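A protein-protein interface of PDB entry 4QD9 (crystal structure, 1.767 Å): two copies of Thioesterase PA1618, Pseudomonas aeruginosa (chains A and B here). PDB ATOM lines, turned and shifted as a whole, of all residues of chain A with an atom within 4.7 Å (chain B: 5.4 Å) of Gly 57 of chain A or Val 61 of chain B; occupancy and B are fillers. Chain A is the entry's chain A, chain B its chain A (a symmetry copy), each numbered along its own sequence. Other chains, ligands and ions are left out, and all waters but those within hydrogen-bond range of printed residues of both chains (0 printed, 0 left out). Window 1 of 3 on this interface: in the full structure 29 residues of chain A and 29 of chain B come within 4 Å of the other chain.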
ATOM      1  N   HIS A  55       7.947  -3.810  -5.742  1.00  0.00           N
ATOM      2  CA  HIS A  55       8.325  -5.220  -5.914  1.00  0.00           C
ATOM      3  C   HIS A  55       7.388  -5.849  -6.947  1.00  0.00           C
ATOM      4  O   HIS A  55       6.162  -5.682  -6.877  1.00  0.00           O
ATOM      5  CB  HIS A  55       8.208  -5.936  -4.553  1.00  0.00           C
ATOM      6  CG  HIS A  55       8.894  -7.265  -4.475  1.00  0.00           C
ATOM      7  ND1 HIS A  55       8.528  -8.345  -5.251  1.00  0.00           N
ATOM      8  CD2 HIS A  55       9.887  -7.707  -3.665  1.00  0.00           C
ATOM      9  CE1 HIS A  55       9.286  -9.385  -4.944  1.00  0.00           C
ATOM     10  NE2 HIS A  55      10.112  -9.028  -3.976  1.00  0.00           N
ATOM     11  N   GLY A  56       7.958  -6.537  -7.930  1.00  0.00           N
ATOM     12  CA  GLY A  56       7.147  -7.147  -8.968  1.00  0.00           C
ATOM     13  C   GLY A  56       6.181  -8.153  -8.376  1.00  0.00           C
ATOM     14  O   GLY A  56       5.063  -8.328  -8.862  1.00  0.00           O
ATOM     15  N   GLY A  57       6.599  -8.812  -7.303  1.00  0.00           N
ATOM     16  CA  GLY A  57       5.716  -9.749  -6.632  1.00  0.00           C
ATOM     17  C   GLY A  57       4.545  -9.054  -5.971  1.00  0.00           C
ATOM     18  O   GLY A  57       3.453  -9.626  -5.855  1.00  0.00           O
ATOM     19  N   ALA A  58       4.757  -7.828  -5.503  1.00  0.00           N
ATOM     20  CA  ALA A  58       3.666  -7.081  -4.877  1.00  0.00           C
ATOM     21  C   ALA A  58       2.582  -6.759  -5.922  1.00  0.00           C
ATOM     22  O   ALA A  58       1.378  -6.803  -5.622  1.00  0.00           O
ATOM     23  CB  ALA A  58       4.188  -5.811  -4.210  1.00  0.00           C
ATOM     24  N   SER A  59       2.995  -6.450  -7.151  1.00  0.00           N
ATOM     25  CA  SER A  59       2.023  -6.266  -8.226  1.00  0.00           C
ATOM     26  C   SER A  59       1.210  -7.539  -8.390  1.00  0.00           C
ATOM     27  O   SER A  59      -0.005  -7.484  -8.620  1.00  0.00           O
ATOM     28  CB  SER A  59       2.703  -5.971  -9.559  1.00  0.00           C
ATOM     29  OG  SER A  59       3.232  -4.670  -9.586  1.00  0.00           O
ATOM     30  N   VAL A  60       1.875  -8.684  -8.253  1.00  0.00           N
ATOM     31  CA  VAL A  60       1.176  -9.954  -8.408  1.00  0.00           C
ATOM     32  C   VAL A  60       0.239 -10.210  -7.227  1.00  0.00           C
ATOM     33  O   VAL A  60      -0.866 -10.729  -7.421  1.00  0.00           O
ATOM     34  CB  VAL A  60       2.145 -11.126  -8.685  1.00  0.00           C
ATOM     35  CG1 VAL A  60       1.386 -12.455  -8.770  1.00  0.00           C
ATOM     36  CG2 VAL A  60       2.896 -10.870 -10.005  1.00  0.00           C
ATOM     37  N   VAL A  61       0.640  -9.831  -6.013  1.00  0.00           N
ATOM     38  CA  VAL A  61      -0.287  -9.934  -4.877  1.00  0.00           C
ATOM     39  C   VAL A  61      -1.562  -9.139  -5.148  1.00  0.00           C
ATOM     40  O   VAL A  61      -2.673  -9.634  -4.919  1.00  0.00           O
ATOM     41  CB  VAL A  61       0.326  -9.429  -3.547  1.00  0.00           C
ATOM     42  CG1 VAL A  61      -0.707  -9.464  -2.428  1.00  0.00           C
ATOM     43  CG2 VAL A  61       1.522 -10.271  -3.164  1.00  0.00           C
ATOM     44  N   ILE B  21       9.339  -5.048   1.237  1.00  0.00           N
ATOM     45  CA  ILE B  21       8.292  -6.045   1.473  1.00  0.00           C
ATOM     46  C   ILE B  21       8.856  -7.344   2.056  1.00  0.00           C
ATOM     47  O   ILE B  21       8.197  -8.009   2.856  1.00  0.00           O
ATOM     48  CB  ILE B  21       7.469  -6.311   0.184  1.00  0.00           C
ATOM     49  CG1 ILE B  21       6.286  -7.246   0.462  1.00  0.00           C
ATOM     50  CG2 ILE B  21       8.345  -6.908  -0.898  1.00  0.00           C
ATOM     51  CD1 ILE B  21       5.311  -7.335  -0.715  1.00  0.00           C
ATOM     52  N   LEU B  25       7.279  -9.373   5.216  1.00  0.00           N
ATOM     53  CA  LEU B  25       6.692 -10.717   5.135  1.00  0.00           C
ATOM     54  C   LEU B  25       7.549 -11.767   5.831  1.00  0.00           C
ATOM     55  O   LEU B  25       7.167 -12.932   5.895  1.00  0.00           O
ATOM     56  CB  LEU B  25       6.453 -11.130   3.677  1.00  0.00           C
ATOM     57  CG  LEU B  25       5.527 -10.238   2.851  1.00  0.00           C
ATOM     58  CD1 LEU B  25       5.326 -10.827   1.459  1.00  0.00           C
ATOM     59  CD2 LEU B  25       4.171 -10.028   3.540  1.00  0.00           C
ATOM     60  N   ILE B  27      10.682 -12.790   4.961  1.00  0.00           N
ATOM     61  CA  ILE B  27      11.520 -13.596   4.074  1.00  0.00           C
ATOM     62  C   ILE B  27      12.934 -13.677   4.638  1.00  0.00           C
ATOM     63  O   ILE B  27      13.494 -12.674   5.077  1.00  0.00           O
ATOM     64  CB  ILE B  27      11.537 -13.023   2.638  1.00  0.00           C
ATOM     65  CG1 ILE B  27      10.153 -13.185   2.011  1.00  0.00           C
ATOM     66  CG2 ILE B  27      12.620 -13.716   1.777  1.00  0.00           C
ATOM     67  CD1 ILE B  27       9.991 -12.486   0.649  1.00  0.00           C
ATOM     68  N   GLY B  57      -0.049 -14.868  -4.451  1.00  0.00           N
ATOM     69  CA  GLY B  57       0.837 -13.756  -4.741  1.00  0.00           C
ATOM     70  C   GLY B  57       2.022 -13.712  -3.801  1.00  0.00           C
ATOM     71  O   GLY B  57       3.111 -13.259  -4.176  1.00  0.00           O
ATOM     72  N   ALA B  58       1.824 -14.150  -2.560  1.00  0.00           N
ATOM     73  CA  ALA B  58       2.929 -14.166  -1.602  1.00  0.00           C
ATOM     74  C   ALA B  58       4.001 -15.177  -2.051  1.00  0.00           C
ATOM     75  O   ALA B  58       5.209 -14.928  -1.907  1.00  0.00           O
ATOM     76  CB  ALA B  58       2.426 -14.479  -0.196  1.00  0.00           C
ATOM     77  N   SER B  59       3.572 -16.309  -2.608  1.00  0.00           N
ATOM     78  CA  SER B  59       4.530 -17.253  -3.180  1.00  0.00           C
ATOM     79  C   SER B  59       5.332 -16.557  -4.266  1.00  0.00           C
ATOM     80  O   SER B  59       6.544 -16.776  -4.391  1.00  0.00           O
ATOM     81  CB  SER B  59       3.832 -18.454  -3.810  1.00  0.00           C
ATOM     82  OG  SER B  59       3.312 -19.315  -2.830  1.00  0.00           O
ATOM     83  N   VAL B  60       4.661 -15.706  -5.038  1.00  0.00           N
ATOM     84  CA  VAL B  60       5.350 -15.003  -6.115  1.00  0.00           C
ATOM     85  C   VAL B  60       6.302 -13.945  -5.557  1.00  0.00           C
ATOM     86  O   VAL B  60       7.400 -13.763  -6.094  1.00  0.00           O
ATOM     87  CB  VAL B  60       4.369 -14.447  -7.172  1.00  0.00           C
ATOM     88  CG1 VAL B  60       5.118 -13.654  -8.250  1.00  0.00           C
ATOM     89  CG2 VAL B  60       3.601 -15.612  -7.823  1.00  0.00           C
ATOM     90  N   VAL B  61       5.920 -13.265  -4.475  1.00  0.00           N
ATOM     91  CA  VAL B  61       6.863 -12.340  -3.829  1.00  0.00           C
ATOM     92  C   VAL B  61       8.140 -13.071  -3.418  1.00  0.00           C
ATOM     93  O   VAL B  61       9.250 -12.583  -3.663  1.00  0.00           O
ATOM     94  CB  VAL B  61       6.273 -11.652  -2.573  1.00  0.00           C
ATOM     95  CG1 VAL B  61       7.322 -10.785  -1.889  1.00  0.00           C
ATOM     96  CG2 VAL B  61       5.077 -10.806  -2.949  1.00  0.00           C
ATOM     97  N   LEU B  62       7.990 -14.229  -2.779  1.00  0.00           N
ATOM     98  CA  LEU B  62       9.171 -15.004  -2.394  1.00  0.00           C
ATOM     99  C   LEU B  62       9.999 -15.376  -3.612  1.00  0.00           C
ATOM    100  O   LEU B  62      11.224 -15.190  -3.617  1.00  0.00           O
ATOM    101  CB  LEU B  62       8.779 -16.263  -1.627  1.00  0.00           C
ATOM    102  CG  LEU B  62       9.882 -17.242  -1.203  1.00  0.00           C
ATOM    103  CD1 LEU B  62      10.963 -16.550  -0.388  1.00  0.00           C
ATOM    104  CD2 LEU B  62       9.268 -18.387  -0.399  1.00  0.00           C
ATOM    105  N   ALA B  63       9.340 -15.865  -4.661  1.00  0.00           N
ATOM    106  CA  ALA B  63      10.069 -16.300  -5.855  1.00  0.00           C
ATOM    107  C   ALA B  63      10.803 -15.141  -6.532  1.00  0.00           C
ATOM    108  O   ALA B  63      11.963 -15.277  -6.956  1.00  0.00           O
ATOM    109  CB  ALA B  63       9.125 -16.993  -6.835  1.00  0.00           C
ATOM    110  N   GLU B  64      10.141 -13.996  -6.627  1.00  0.00           N
ATOM    111  CA  GLU B  64      10.759 -12.854  -7.298  1.00  0.00           C
ATOM    112  C   GLU B  64      11.835 -12.188  -6.415  1.00  0.00           C
ATOM    113  O   GLU B  64      12.828 -11.681  -6.935  1.00  0.00           O
ATOM    114  CB  GLU B  64       9.694 -11.854  -7.801  1.00  0.00           C
ATOM    115  CG  GLU B  64      10.283 -10.670  -8.584  1.00  0.00           C
ATOM    116  CD  GLU B  64       9.354 -10.101  -9.660  1.00  0.00           C
ATOM    117  OE1 GLU B  64       8.390 -10.786 -10.112  1.00  0.00           O
ATOM    118  OE2 GLU B  64       9.600  -8.945 -10.058  1.00  0.00           O
ATOM    119  N   SER B  65      11.657 -12.206  -5.093  1.00  0.00           N
ATOM    120  CA  SER B  65      12.707 -11.720  -4.189  1.00  0.00           C
ATOM    121  C   SER B  65      13.958 -12.561  -4.369  1.00  0.00           C
ATOM    122  O   SER B  65      15.071 -12.035  -4.468  1.00  0.00           O
ATOM    123  CB  SER B  65      12.279 -11.807  -2.722  1.00  0.00           C
ATOM    124  OG  SER B  65      11.616 -10.644  -2.300  1.00  0.00           O
ATOM    125  N   LEU B  66      13.760 -13.874  -4.380  1.00  0.00           N
ATOM    126  CA  LEU B  66      14.855 -14.831  -4.467  1.00  0.00           C
ATOM    127  C   LEU B  66      15.585 -14.704  -5.802  1.00  0.00           C
ATOM    128  O   LEU B  66      16.809 -14.551  -5.840  1.00  0.00           O
ATOM    129  CB  LEU B  66      14.315 -16.254  -4.291  1.00  0.00           C
ATOM    130  CG  LEU B  66      15.332 -17.390  -4.218  1.00  0.00           C
ATOM    131  CD1 LEU B  66      16.431 -17.076  -3.207  1.00  0.00           C
ATOM    132  CD2 LEU B  66      14.641 -18.704  -3.883  1.00  0.00           C
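Gly 57 of chain A touches Val 61 of chain B, and with the chains exchanged Val 61 of chain A touches Gly 57 of chain B. Ala 58 of chain A touches Val 61 of chain B, and with the chains exchanged Val 61 of chain A touches Ala 58 of chain B. Val 60 of chain A touches its own counterpart, Val 60 of chain B. Val 61 of chain B touches its own counterpart, Val 61 of chain A. Of the 13 pairs that touch across the chains among the printed residues, 6 have their exchanged pair printed and touching as well.
Of the 13 printed residues of chain B, 7 touch a printed residue of chain A. Printed residues of chain B that touch a printed residue of chain A: Ile 21, Gly 57, Ala 58, Val 60, Val 61, Glu 64 and Ser 65. Hydrophobic or aromatic side chains of chain B that line the printed part of chain A: Ile 21, Val 60 and Val 61. Of the 7 printed residues of chain A, 6 touch a printed residue of chain B. Hydrophobic or aromatic side chains of chain A that line the printed part of chain B: His 55, Ala 58, Val 60 and Val 61. Among the printed residues, no Asp or Glu carboxylate lies within 4 Å of a Lys or Arg side-chain nitrogen of the other chain.
Of the printed residues of chain B, Gly 57 of chain A touches Val 61 and Glu 64. Val 61 of chain B touches four residues of chain A. Of the printed residues of chain A, Gly 57 of chain B touches Val 61 (3.5 Å). Printed residues of chain B within 4 Å of Val 60 of chain A: Val 60. Of the printed residues of chain B, His 55 of chain A touches Ile 21, Val 61, Glu 64 and Ser 65. Printed residues of chain A within 4 Å of Glu 64 of chain B: His 55, Gly 56 and Gly 57. Ser 59 of chain B touches none of the printed residues of chain A. The nearest printed residue of chain B that does not touch Gly 57 of chain A is Gly 57 of chain B (4.02 Å). The nearest printed residue of chain A that does not touch Val 61 of chain B is Val 60 of chain A (6.0 Å).
Among the printed residues, pairs that only touch across the chains: His 55 of chain A with Ile 21 of chain B (3.3 Å), His 55 of chain A with Val 61 of chain B (3.4 Å), His 55 of chain A with Glu 64 of chain B (3.8 Å), Gly 56 of chain A with Glu 64 of chain B (3.2 Å), Gly 57 of chain A with Val 61 of chain B (3.5 Å), Gly 57 of chain A with Glu 64 of chain B (3.8 Å), Ala 58 of chain A with Ile 21 of chain B (3.97 Å), Ala 58 of chain A with Val 61 of chain B (3.9 Å), Val 60 of chain A with Val 60 of chain B (3.9 Å), Val 61 of chain A with Gly 57 of chain B (3.5 Å), Val 61 of chain A with Ala 58 of chain B (3.9 Å) and Val 61 of chain A with Val 61 of chain B (3.6 Å).
N of Gly 57 of chain A lies within hydrogen-bond range of ND1 of His 55 of chain A. The side-chain hydroxyl of Ser 65 of chain B lies close to the backbone carbonyl oxygen of Val 61 of chain B (3.3 Å).
NE2 of His 55 of chain A is in hydrogen-bond range of OG of Ser 65 of chain B, 2.8 Å away.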
